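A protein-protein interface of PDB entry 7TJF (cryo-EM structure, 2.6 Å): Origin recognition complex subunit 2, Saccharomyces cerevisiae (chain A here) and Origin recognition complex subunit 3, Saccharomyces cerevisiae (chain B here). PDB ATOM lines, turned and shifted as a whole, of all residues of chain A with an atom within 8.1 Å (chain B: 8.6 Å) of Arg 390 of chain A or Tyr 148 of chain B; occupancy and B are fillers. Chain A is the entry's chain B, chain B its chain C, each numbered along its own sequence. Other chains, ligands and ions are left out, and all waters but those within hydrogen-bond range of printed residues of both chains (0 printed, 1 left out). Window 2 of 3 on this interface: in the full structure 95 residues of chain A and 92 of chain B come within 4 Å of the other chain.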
ATOM      1  N   GLU A 387     -34.539  26.614 -27.932  1.00  0.00           N
ATOM      2  CA  GLU A 387     -34.334  25.415 -28.728  1.00  0.00           C
ATOM      3  C   GLU A 387     -33.239  24.548 -28.112  1.00  0.00           C
ATOM      4  O   GLU A 387     -32.414  25.007 -27.317  1.00  0.00           O
ATOM      5  CB  GLU A 387     -33.975  25.750 -30.184  1.00  0.00           C
ATOM      6  CG  GLU A 387     -32.953  26.881 -30.452  1.00  0.00           C
ATOM      7  CD  GLU A 387     -33.504  28.297 -30.297  1.00  0.00           C
ATOM      8  OE1 GLU A 387     -33.874  28.681 -29.168  1.00  0.00           O
ATOM      9  OE2 GLU A 387     -33.555  29.026 -31.310  1.00  0.00           O
ATOM     10  N   LEU A 388     -33.250  23.270 -28.480  1.00  0.00           N
ATOM     11  CA  LEU A 388     -32.268  22.333 -27.954  1.00  0.00           C
ATOM     12  C   LEU A 388     -30.898  22.580 -28.572  1.00  0.00           C
ATOM     13  O   LEU A 388     -30.778  22.862 -29.768  1.00  0.00           O
ATOM     14  CB  LEU A 388     -32.704  20.894 -28.226  1.00  0.00           C
ATOM     15  CG  LEU A 388     -34.015  20.387 -27.622  1.00  0.00           C
ATOM     16  CD1 LEU A 388     -34.607  19.296 -28.499  1.00  0.00           C
ATOM     17  CD2 LEU A 388     -33.804  19.878 -26.207  1.00  0.00           C
ATOM     18  N   THR A 389     -29.860  22.471 -27.749  1.00  0.00           N
ATOM     19  CA  THR A 389     -28.499  22.435 -28.263  1.00  0.00           C
ATOM     20  C   THR A 389     -28.181  21.027 -28.759  1.00  0.00           C
ATOM     21  O   THR A 389     -29.005  20.112 -28.679  1.00  0.00           O
ATOM     22  CB  THR A 389     -27.505  22.894 -27.198  1.00  0.00           C
ATOM     23  OG1 THR A 389     -27.287  21.843 -26.250  1.00  0.00           O
ATOM     24  CG2 THR A 389     -28.012  24.138 -26.487  1.00  0.00           C
ATOM     25  N   ARG A 390     -26.970  20.847 -29.291  1.00  0.00           N
ATOM     26  CA  ARG A 390     -26.626  19.574 -29.917  1.00  0.00           C
ATOM     27  C   ARG A 390     -26.443  18.459 -28.893  1.00  0.00           C
ATOM     28  O   ARG A 390     -26.768  17.303 -29.179  1.00  0.00           O
ATOM     29  CB  ARG A 390     -25.368  19.718 -30.768  1.00  0.00           C
ATOM     30  CG  ARG A 390     -25.420  18.860 -32.010  1.00  0.00           C
ATOM     31  CD  ARG A 390     -24.088  18.789 -32.729  1.00  0.00           C
ATOM     32  NE  ARG A 390     -23.740  17.420 -33.095  1.00  0.00           N
ATOM     33  CZ  ARG A 390     -24.237  16.765 -34.137  1.00  0.00           C
ATOM     34  NH1 ARG A 390     -25.119  17.322 -34.951  1.00  0.00           N
ATOM     35  NH2 ARG A 390     -23.835  15.519 -34.371  1.00  0.00           N
ATOM     36  N   SER A 391     -25.935  18.781 -27.702  1.00  0.00           N
ATOM     37  CA  SER A 391     -25.787  17.768 -26.667  1.00  0.00           C
ATOM     38  C   SER A 391     -27.121  17.379 -26.039  1.00  0.00           C
ATOM     39  O   SER A 391     -27.219  16.295 -25.455  1.00  0.00           O
ATOM     40  CB  SER A 391     -24.822  18.258 -25.588  1.00  0.00           C
ATOM     41  OG  SER A 391     -24.810  17.381 -24.476  1.00  0.00           O
ATOM     42  N   GLU A 392     -28.144  18.230 -26.145  1.00  0.00           N
ATOM     43  CA  GLU A 392     -29.460  17.922 -25.601  1.00  0.00           C
ATOM     44  C   GLU A 392     -30.337  17.117 -26.549  1.00  0.00           C
ATOM     45  O   GLU A 392     -31.371  16.598 -26.115  1.00  0.00           O
ATOM     46  CB  GLU A 392     -30.198  19.207 -25.209  1.00  0.00           C
ATOM     47  CG  GLU A 392     -29.770  19.789 -23.872  1.00  0.00           C
ATOM     48  CD  GLU A 392     -29.949  21.292 -23.806  1.00  0.00           C
ATOM     49  OE1 GLU A 392     -29.881  21.945 -24.864  1.00  0.00           O
ATOM     50  OE2 GLU A 392     -30.156  21.822 -22.695  1.00  0.00           O
ATOM     51  N   THR A 393     -29.962  16.994 -27.824  1.00  0.00           N
ATOM     52  CA  THR A 393     -30.732  16.179 -28.755  1.00  0.00           C
ATOM     53  C   THR A 393     -30.485  14.689 -28.574  1.00  0.00           C
ATOM     54  O   THR A 393     -31.244  13.891 -29.137  1.00  0.00           O
ATOM     55  CB  THR A 393     -30.423  16.565 -30.206  1.00  0.00           C
ATOM     56  OG1 THR A 393     -29.021  16.408 -30.461  1.00  0.00           O
ATOM     57  CG2 THR A 393     -30.833  18.001 -30.478  1.00  0.00           C
ATOM     58  N   LYS A 394     -29.441  14.320 -27.818  1.00  0.00           N
ATOM     59  CA  LYS A 394     -29.081  12.943 -27.451  1.00  0.00           C
ATOM     60  C   LYS A 394     -28.755  12.171 -28.724  1.00  0.00           C
ATOM     61  O   LYS A 394     -27.873  12.612 -29.481  1.00  0.00           O
ATOM     62  CB  LYS A 394     -30.176  12.336 -26.564  1.00  0.00           C
ATOM     63  CG  LYS A 394     -30.572  13.201 -25.381  1.00  0.00           C
ATOM     64  CD  LYS A 394     -29.866  12.767 -24.116  1.00  0.00           C
ATOM     65  CE  LYS A 394     -30.667  11.709 -23.382  1.00  0.00           C
ATOM     66  NZ  LYS A 394     -31.660  12.321 -22.461  1.00  0.00           N
ATOM     67  N   TYR A 395     -29.405  11.045 -28.999  1.00  0.00           N
ATOM     68  CA  TYR A 395     -29.098  10.231 -30.172  1.00  0.00           C
ATOM     69  C   TYR A 395     -30.420   9.635 -30.645  1.00  0.00           C
ATOM     70  O   TYR A 395     -30.858   8.612 -30.109  1.00  0.00           O
ATOM     71  CB  TYR A 395     -28.077   9.153 -29.834  1.00  0.00           C
ATOM     72  CG  TYR A 395     -27.474   8.462 -31.033  1.00  0.00           C
ATOM     73  CD1 TYR A 395     -26.342   8.973 -31.656  1.00  0.00           C
ATOM     74  CD2 TYR A 395     -28.034   7.294 -31.540  1.00  0.00           C
ATOM     75  CE1 TYR A 395     -25.785   8.343 -32.751  1.00  0.00           C
ATOM     76  CE2 TYR A 395     -27.484   6.659 -32.636  1.00  0.00           C
ATOM     77  CZ  TYR A 395     -26.360   7.188 -33.235  1.00  0.00           C
ATOM     78  OH  TYR A 395     -25.810   6.563 -34.324  1.00  0.00           O
ATOM     79  N   TRP A 396     -31.035  10.288 -31.640  1.00  0.00           N
ATOM     80  CA  TRP A 396     -32.390   9.989 -32.126  1.00  0.00           C
ATOM     81  C   TRP A 396     -33.417  10.001 -30.993  1.00  0.00           C
ATOM     82  O   TRP A 396     -34.283   9.131 -30.898  1.00  0.00           O
ATOM     83  CB  TRP A 396     -32.440   8.663 -32.888  1.00  0.00           C
ATOM     84  CG  TRP A 396     -32.219   8.796 -34.354  1.00  0.00           C
ATOM     85  CD1 TRP A 396     -33.173   8.893 -35.320  1.00  0.00           C
ATOM     86  CD2 TRP A 396     -30.960   8.827 -35.028  1.00  0.00           C
ATOM     87  NE1 TRP A 396     -32.588   8.991 -36.555  1.00  0.00           N
ATOM     88  CE2 TRP A 396     -31.227   8.953 -36.404  1.00  0.00           C
ATOM     89  CE3 TRP A 396     -29.630   8.766 -34.602  1.00  0.00           C
ATOM     90  CZ2 TRP A 396     -30.216   9.017 -37.358  1.00  0.00           C
ATOM     91  CZ3 TRP A 396     -28.629   8.829 -35.550  1.00  0.00           C
ATOM     92  CH2 TRP A 396     -28.928   8.951 -36.911  1.00  0.00           C
ATOM     93  N   HIS A 399     -37.604  14.824 -29.625  1.00  0.00           N
ATOM     94  CA  HIS A 399     -37.280  16.233 -29.424  1.00  0.00           C
ATOM     95  C   HIS A 399     -38.343  16.953 -28.607  1.00  0.00           C
ATOM     96  O   HIS A 399     -38.021  17.904 -27.887  1.00  0.00           O
ATOM     97  CB  HIS A 399     -37.096  16.928 -30.771  1.00  0.00           C
ATOM     98  CG  HIS A 399     -35.799  16.605 -31.444  1.00  0.00           C
ATOM     99  ND1 HIS A 399     -35.383  17.238 -32.595  1.00  0.00           N
ATOM    100  CD2 HIS A 399     -34.828  15.717 -31.129  1.00  0.00           C
ATOM    101  CE1 HIS A 399     -34.209  16.754 -32.959  1.00  0.00           C
ATOM    102  NE2 HIS A 399     -33.850  15.830 -32.086  1.00  0.00           N
ATOM    103  N   VAL B 127     -16.650   8.662 -17.299  1.00  0.00           N
ATOM    104  CA  VAL B 127     -17.759   8.917 -18.212  1.00  0.00           C
ATOM    105  C   VAL B 127     -18.983   8.155 -17.730  1.00  0.00           C
ATOM    106  O   VAL B 127     -18.921   6.938 -17.512  1.00  0.00           O
ATOM    107  CB  VAL B 127     -17.403   8.530 -19.657  1.00  0.00           C
ATOM    108  CG1 VAL B 127     -18.544   8.883 -20.598  1.00  0.00           C
ATOM    109  CG2 VAL B 127     -16.125   9.224 -20.086  1.00  0.00           C
ATOM    110  N   ILE B 129     -22.999   7.073 -18.335  1.00  0.00           N
ATOM    111  CA  ILE B 129     -23.861   6.764 -19.476  1.00  0.00           C
ATOM    112  C   ILE B 129     -25.232   6.354 -18.951  1.00  0.00           C
ATOM    113  O   ILE B 129     -25.364   5.310 -18.305  1.00  0.00           O
ATOM    114  CB  ILE B 129     -23.259   5.652 -20.352  1.00  0.00           C
ATOM    115  CG1 ILE B 129     -21.950   6.116 -20.996  1.00  0.00           C
ATOM    116  CG2 ILE B 129     -24.247   5.185 -21.414  1.00  0.00           C
ATOM    117  CD1 ILE B 129     -20.853   5.084 -20.948  1.00  0.00           C
ATOM    118  N   MET B 141     -28.378  -0.662 -30.686  1.00  0.00           N
ATOM    119  CA  MET B 141     -28.698   0.709 -30.300  1.00  0.00           C
ATOM    120  C   MET B 141     -28.103   1.079 -28.947  1.00  0.00           C
ATOM    121  O   MET B 141     -27.675   2.223 -28.756  1.00  0.00           O
ATOM    122  CB  MET B 141     -30.213   0.922 -30.301  1.00  0.00           C
ATOM    123  CG  MET B 141     -30.869   1.079 -31.681  1.00  0.00           C
ATOM    124  SD  MET B 141     -29.855   1.667 -33.067  1.00  0.00           S
ATOM    125  CE  MET B 141     -29.475   3.367 -32.604  1.00  0.00           C
ATOM    126  N   MET B 142     -28.062   0.125 -28.009  1.00  0.00           N
ATOM    127  CA  MET B 142     -27.403   0.343 -26.722  1.00  0.00           C
ATOM    128  C   MET B 142     -25.927   0.670 -26.902  1.00  0.00           C
ATOM    129  O   MET B 142     -25.428   1.653 -26.339  1.00  0.00           O
ATOM    130  CB  MET B 142     -27.560  -0.891 -25.832  1.00  0.00           C
ATOM    131  CG  MET B 142     -28.976  -1.229 -25.425  1.00  0.00           C
ATOM    132  SD  MET B 142     -28.990  -2.475 -24.118  1.00  0.00           S
ATOM    133  CE  MET B 142     -29.020  -1.469 -22.645  1.00  0.00           C
ATOM    134  N   LEU B 143     -25.227  -0.114 -27.731  1.00  0.00           N
ATOM    135  CA  LEU B 143     -23.806   0.142 -27.948  1.00  0.00           C
ATOM    136  C   LEU B 143     -23.579   1.441 -28.718  1.00  0.00           C
ATOM    137  O   LEU B 143     -22.667   2.202 -28.387  1.00  0.00           O
ATOM    138  CB  LEU B 143     -23.142  -1.032 -28.670  1.00  0.00           C
ATOM    139  CG  LEU B 143     -21.619  -0.849 -28.760  1.00  0.00           C
ATOM    140  CD1 LEU B 143     -21.000  -0.803 -27.369  1.00  0.00           C
ATOM    141  CD2 LEU B 143     -20.934  -1.883 -29.611  1.00  0.00           C
ATOM    142  N   ARG B 144     -24.415   1.730 -29.721  1.00  0.00           N
ATOM    143  CA  ARG B 144     -24.213   2.937 -30.523  1.00  0.00           C
ATOM    144  C   ARG B 144     -24.471   4.203 -29.711  1.00  0.00           C
ATOM    145  O   ARG B 144     -23.686   5.158 -29.787  1.00  0.00           O
ATOM    146  CB  ARG B 144     -25.092   2.898 -31.772  1.00  0.00           C
ATOM    147  CG  ARG B 144     -24.573   1.947 -32.841  1.00  0.00           C
ATOM    148  CD  ARG B 144     -25.322   2.093 -34.160  1.00  0.00           C
ATOM    149  NE  ARG B 144     -25.004   3.339 -34.849  1.00  0.00           N
ATOM    150  CZ  ARG B 144     -23.890   3.566 -35.535  1.00  0.00           C
ATOM    151  NH1 ARG B 144     -22.959   2.636 -35.674  1.00  0.00           N
ATOM    152  NH2 ARG B 144     -23.706   4.757 -36.094  1.00  0.00           N
ATOM    153  N   ARG B 145     -25.528   4.208 -28.887  1.00  0.00           N
ATOM    154  CA  ARG B 145     -25.785   5.352 -28.018  1.00  0.00           C
ATOM    155  C   ARG B 145     -24.714   5.487 -26.943  1.00  0.00           C
ATOM    156  O   ARG B 145     -24.277   6.608 -26.644  1.00  0.00           O
ATOM    157  CB  ARG B 145     -27.175   5.238 -27.391  1.00  0.00           C
ATOM    158  CG  ARG B 145     -28.296   5.444 -28.387  1.00  0.00           C
ATOM    159  CD  ARG B 145     -29.660   5.455 -27.731  1.00  0.00           C
ATOM    160  NE  ARG B 145     -30.643   6.096 -28.595  1.00  0.00           N
ATOM    161  CZ  ARG B 145     -31.522   5.447 -29.344  1.00  0.00           C
ATOM    162  NH1 ARG B 145     -31.608   4.128 -29.324  1.00  0.00           N
ATOM    163  NH2 ARG B 145     -32.337   6.140 -30.133  1.00  0.00           N
ATOM    164  N   SER B 146     -24.251   4.359 -26.384  1.00  0.00           N
ATOM    165  CA  SER B 146     -23.218   4.397 -25.353  1.00  0.00           C
ATOM    166  C   SER B 146     -21.895   4.927 -25.894  1.00  0.00           C
ATOM    167  O   SER B 146     -21.252   5.761 -25.250  1.00  0.00           O
ATOM    168  CB  SER B 146     -23.030   3.005 -24.754  1.00  0.00           C
ATOM    169  OG  SER B 146     -24.275   2.443 -24.382  1.00  0.00           O
ATOM    170  N   MET B 147     -21.486   4.487 -27.085  1.00  0.00           N
ATOM    171  CA  MET B 147     -20.223   4.972 -27.628  1.00  0.00           C
ATOM    172  C   MET B 147     -20.329   6.383 -28.182  1.00  0.00           C
ATOM    173  O   MET B 147     -19.337   7.116 -28.140  1.00  0.00           O
ATOM    174  CB  MET B 147     -19.676   4.020 -28.695  1.00  0.00           C
ATOM    175  CG  MET B 147     -19.481   2.542 -28.292  1.00  0.00           C
ATOM    176  SD  MET B 147     -18.196   2.076 -27.098  1.00  0.00           S
ATOM    177  CE  MET B 147     -18.917   2.380 -25.481  1.00  0.00           C
ATOM    178  N   TYR B 148     -21.505   6.796 -28.675  1.00  0.00           N
ATOM    179  CA  TYR B 148     -21.680   8.198 -29.041  1.00  0.00           C
ATOM    180  C   TYR B 148     -21.577   9.103 -27.820  1.00  0.00           C
ATOM    181  O   TYR B 148     -20.909  10.142 -27.872  1.00  0.00           O
ATOM    182  CB  TYR B 148     -23.016   8.418 -29.748  1.00  0.00           C
ATOM    183  CG  TYR B 148     -23.282   9.881 -30.030  1.00  0.00           C
ATOM    184  CD1 TYR B 148     -22.566  10.557 -31.014  1.00  0.00           C
ATOM    185  CD2 TYR B 148     -24.233  10.594 -29.302  1.00  0.00           C
ATOM    186  CE1 TYR B 148     -22.791  11.896 -31.268  1.00  0.00           C
ATOM    187  CE2 TYR B 148     -24.466  11.932 -29.553  1.00  0.00           C
ATOM    188  CZ  TYR B 148     -23.743  12.578 -30.535  1.00  0.00           C
ATOM    189  OH  TYR B 148     -23.973  13.909 -30.787  1.00  0.00           O
ATOM    190  N   LYS B 149     -22.202   8.705 -26.705  1.00  0.00           N
ATOM    191  CA  LYS B 149     -22.112   9.496 -25.481  1.00  0.00           C
ATOM    192  C   LYS B 149     -20.699   9.486 -24.909  1.00  0.00           C
ATOM    193  O   LYS B 149     -20.225  10.509 -24.404  1.00  0.00           O
ATOM    194  CB  LYS B 149     -23.119   8.988 -24.450  1.00  0.00           C
ATOM    195  CG  LYS B 149     -24.535   9.482 -24.693  1.00  0.00           C
ATOM    196  CD  LYS B 149     -25.497   8.986 -23.630  1.00  0.00           C
ATOM    197  CE  LYS B 149     -25.846   7.525 -23.843  1.00  0.00           C
ATOM    198  NZ  LYS B 149     -27.314   7.293 -23.835  1.00  0.00           N
ATOM    199  N   LEU B 150     -20.005   8.348 -25.011  1.00  0.00           N
ATOM    200  CA  LEU B 150     -18.628   8.248 -24.537  1.00  0.00           C
ATOM    201  C   LEU B 150     -17.689   9.136 -25.350  1.00  0.00           C
ATOM    202  O   LEU B 150     -16.868   9.867 -24.782  1.00  0.00           O
ATOM    203  CB  LEU B 150     -18.175   6.789 -24.590  1.00  0.00           C
ATOM    204  CG  LEU B 150     -16.674   6.517 -24.488  1.00  0.00           C
ATOM    205  CD1 LEU B 150     -16.182   6.851 -23.099  1.00  0.00           C
ATOM    206  CD2 LEU B 150     -16.354   5.080 -24.846  1.00  0.00           C
ATOM    207  N   TYR B 151     -17.817   9.100 -26.681  1.00  0.00           N
ATOM    208  CA  TYR B 151     -16.983   9.929 -27.546  1.00  0.00           C
ATOM    209  C   TYR B 151     -17.299  11.410 -27.378  1.00  0.00           C
ATOM    210  O   TYR B 151     -16.386  12.244 -27.383  1.00  0.00           O
ATOM    211  CB  TYR B 151     -17.158   9.509 -29.004  1.00  0.00           C
ATOM    212  CG  TYR B 151     -16.103  10.072 -29.926  1.00  0.00           C
ATOM    213  CD1 TYR B 151     -14.755   9.827 -29.700  1.00  0.00           C
ATOM    214  CD2 TYR B 151     -16.455  10.853 -31.019  1.00  0.00           C
ATOM    215  CE1 TYR B 151     -13.786  10.340 -30.538  1.00  0.00           C
ATOM    216  CE2 TYR B 151     -15.493  11.369 -31.864  1.00  0.00           C
ATOM    217  CZ  TYR B 151     -14.160  11.111 -31.617  1.00  0.00           C
ATOM    218  OH  TYR B 151     -13.195  11.619 -32.453  1.00  0.00           O
ATOM    219  N   SER B 152     -18.582  11.754 -27.212  1.00  0.00           N
ATOM    220  CA  SER B 152     -18.969  13.145 -26.999  1.00  0.00           C
ATOM    221  C   SER B 152     -18.457  13.673 -25.664  1.00  0.00           C
ATOM    222  O   SER B 152     -17.979  14.810 -25.586  1.00  0.00           O
ATOM    223  CB  SER B 152     -20.488  13.281 -27.079  1.00  0.00           C
ATOM    224  OG  SER B 152     -20.985  12.759 -28.296  1.00  0.00           O
ATOM    225  N   ALA B 153     -18.539  12.859 -24.607  1.00  0.00           N
ATOM    226  CA  ALA B 153     -18.049  13.283 -23.301  1.00  0.00           C
ATOM    227  C   ALA B 153     -16.529  13.380 -23.281  1.00  0.00           C
ATOM    228  O   ALA B 153     -15.968  14.256 -22.615  1.00  0.00           O
ATOM    229  CB  ALA B 153     -18.541  12.323 -22.219  1.00  0.00           C
ATOM    230  N   ALA B 154     -15.845  12.490 -24.005  1.00  0.00           N
ATOM    231  CA  ALA B 154     -14.392  12.569 -24.081  1.00  0.00           C
ATOM    232  C   ALA B 154     -13.933  13.756 -24.919  1.00  0.00           C
ATOM    233  O   ALA B 154     -12.888  14.348 -24.628  1.00  0.00           O
ATOM    234  CB  ALA B 154     -13.826  11.265 -24.639  1.00  0.00           C
ATOM    235  N   ASP B 155     -14.690  14.115 -25.959  1.00  0.00           N
ATOM    236  CA  ASP B 155     -14.335  15.272 -26.773  1.00  0.00           C
ATOM    237  C   ASP B 155     -14.694  16.589 -26.096  1.00  0.00           C
ATOM    238  O   ASP B 155     -14.053  17.610 -26.368  1.00  0.00           O
ATOM    239  CB  ASP B 155     -15.020  15.182 -28.136  1.00  0.00           C
ATOM    240  CG  ASP B 155     -14.443  16.157 -29.142  1.00  0.00           C
ATOM    241  OD1 ASP B 155     -13.321  15.911 -29.633  1.00  0.00           O
ATOM    242  OD2 ASP B 155     -15.110  17.171 -29.437  1.00  0.00           O
ATOM    243  N   ASP B 180     -13.723  11.554 -37.309  1.00  0.00           N
ATOM    244  CA  ASP B 180     -14.840  10.761 -36.828  1.00  0.00           C
ATOM    245  C   ASP B 180     -14.406   9.319 -36.575  1.00  0.00           C
ATOM    246  O   ASP B 180     -13.415   8.832 -37.123  1.00  0.00           O
ATOM    247  CB  ASP B 180     -15.990  10.797 -37.834  1.00  0.00           C
ATOM    248  CG  ASP B 180     -16.351  12.207 -38.253  1.00  0.00           C
ATOM    249  OD1 ASP B 180     -16.885  12.960 -37.414  1.00  0.00           O
ATOM    250  OD2 ASP B 180     -16.106  12.561 -39.425  1.00  0.00           O
ATOM    251  N   VAL B 181     -15.168   8.633 -35.720  1.00  0.00           N
ATOM    252  CA  VAL B 181     -14.876   7.262 -35.328  1.00  0.00           C
ATOM    253  C   VAL B 181     -16.123   6.410 -35.519  1.00  0.00           C
ATOM    254  O   VAL B 181     -17.236   6.916 -35.677  1.00  0.00           O
ATOM    255  CB  VAL B 181     -14.387   7.152 -33.865  1.00  0.00           C
ATOM    256  CG1 VAL B 181     -13.043   7.841 -33.685  1.00  0.00           C
ATOM    257  CG2 VAL B 181     -15.428   7.726 -32.910  1.00  0.00           C
ATOM    258  N   SER B 182     -15.919   5.098 -35.504  1.00  0.00           N
ATOM    259  CA  SER B 182     -17.032   4.161 -35.499  1.00  0.00           C
ATOM    260  C   SER B 182     -17.558   3.985 -34.080  1.00  0.00           C
ATOM    261  O   SER B 182     -16.786   3.839 -33.129  1.00  0.00           O
ATOM    262  CB  SER B 182     -16.600   2.815 -36.075  1.00  0.00           C
ATOM    263  OG  SER B 182     -17.643   1.862 -35.982  1.00  0.00           O
ATOM    264  N   TYR B 183     -18.884   4.006 -33.938  1.00  0.00           N
ATOM    265  CA  TYR B 183     -19.516   3.936 -32.621  1.00  0.00           C
ATOM    266  C   TYR B 183     -19.723   2.471 -32.254  1.00  0.00           C
ATOM    267  O   TYR B 183     -20.820   1.914 -32.320  1.00  0.00           O
ATOM    268  CB  TYR B 183     -20.809   4.739 -32.607  1.00  0.00           C
ATOM    269  CG  TYR B 183     -20.544   6.212 -32.780  1.00  0.00           C
ATOM    270  CD1 TYR B 183     -19.466   6.814 -32.137  1.00  0.00           C
ATOM    271  CD2 TYR B 183     -21.344   6.995 -33.600  1.00  0.00           C
ATOM    272  CE1 TYR B 183     -19.202   8.156 -32.295  1.00  0.00           C
ATOM    273  CE2 TYR B 183     -21.087   8.339 -33.768  1.00  0.00           C
ATOM    274  CZ  TYR B 183     -20.013   8.914 -33.111  1.00  0.00           C
ATOM    275  OH  TYR B 183     -19.746  10.252 -33.268  1.00  0.00           O
ATOM    276  N   ASP B 184     -18.620   1.846 -31.859  1.00  0.00           N
ATOM    277  CA  ASP B 184     -18.586   0.450 -31.460  1.00  0.00           C
ATOM    278  C   ASP B 184     -17.523   0.301 -30.377  1.00  0.00           C
ATOM    279  O   ASP B 184     -16.891   1.277 -29.967  1.00  0.00           O
ATOM    280  CB  ASP B 184     -18.422  -0.444 -32.709  1.00  0.00           C
ATOM    281  CG  ASP B 184     -17.069  -0.283 -33.428  1.00  0.00           C
ATOM    282  OD1 ASP B 184     -15.984  -0.227 -32.825  1.00  0.00           O
ATOM    283  OD2 ASP B 184     -17.102  -0.155 -34.661  1.00  0.00           O
ATOM    284  N   LEU B 187     -13.807   1.771 -30.040  1.00  0.00           N
ATOM    285  CA  LEU B 187     -13.545   3.060 -29.407  1.00  0.00           C
ATOM    286  C   LEU B 187     -13.010   2.874 -27.992  1.00  0.00           C
ATOM    287  O   LEU B 187     -12.159   3.645 -27.532  1.00  0.00           O
ATOM    288  CB  LEU B 187     -14.822   3.903 -29.402  1.00  0.00           C
ATOM    289  CG  LEU B 187     -14.863   5.206 -28.599  1.00  0.00           C
ATOM    290  CD1 LEU B 187     -13.862   6.208 -29.145  1.00  0.00           C
ATOM    291  CD2 LEU B 187     -16.264   5.791 -28.594  1.00  0.00           C
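The side-chain hydroxyl (OH) of Tyr 395 of chain A lies within hydrogen-bond range of the guanidinium group (NH2) of Arg 144 of chain B (3.3 Å).
O of Tyr 395 of chain A lies within hydrogen-bond range of NH2 of Arg 145 of chain B (2.9 Å).
The backbone carbonyl oxygen (O) of Arg 390 of chain A lies within hydrogen-bond range of the side-chain hydroxyl (OG1) of Thr 393 of chain A (2.7 Å).
The side-chain hydroxyl (OG) of Ser 152 of chain B lies within hydrogen-bond range of the backbone carbonyl oxygen (O) of Tyr 148 of chain B.
Among the printed residues, merely in contact across the chains: Arg 390 of chain A with Tyr 148 of chain B, Lys 394 of chain A with Tyr 148 of chain B, Tyr 395 of chain A with Met 141 of chain B, Tyr 395 of chain A with Tyr 148 of chain B and Trp 396 of chain A with Arg 145 of chain B.
Tyr 148 of chain B touches just these residues of chain A: Arg 390, Lys 394 and Tyr 395.
No residue of chain B comes within 4 Å of Thr 389 of chain A.
Printed residues of chain B within 4 Å of Tyr 395 of chain A: Met 141, Arg 144, Arg 145 and Tyr 148.
Of the printed residues of chain A, Arg 145 of chain B touches Tyr 395 (2.9 Å) and Trp 396 (3.6 Å).
Of the printed residues of chain A, Met 141 of chain B touches Tyr 395 (3.8 Å).
Of the printed residues of chain A, Arg 144 of chain B touches Tyr 395 (3.3 Å).
Printed residues of chain B within 4 Å of Trp 396 of chain A: Arg 145 (3.6 Å).
The nearest residue of chain A that does not touch Tyr 148 of chain B is Thr 393 of chain A (5.6 Å).
The nearest printed residue of chain B that does not touch Trp 396 of chain A is Met 141 of chain B (5.8 Å).
Of the 11 printed residues of chain A, 4 touch a printed residue of chain B.
Printed residues of chain A that touch a printed residue of chain B: Arg 390, Lys 394, Tyr 395 and Trp 396.
Hydrophobic or aromatic side chains of chain A that line the printed part of chain B: Tyr 395 and Trp 396.
Of the 23 printed residues of chain B, 4 touch a printed residue of chain A.
Among the printed residues, no Asp or Glu carboxylate lies within 4 Å of a Lys or Arg side-chain nitrogen of the other chain.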
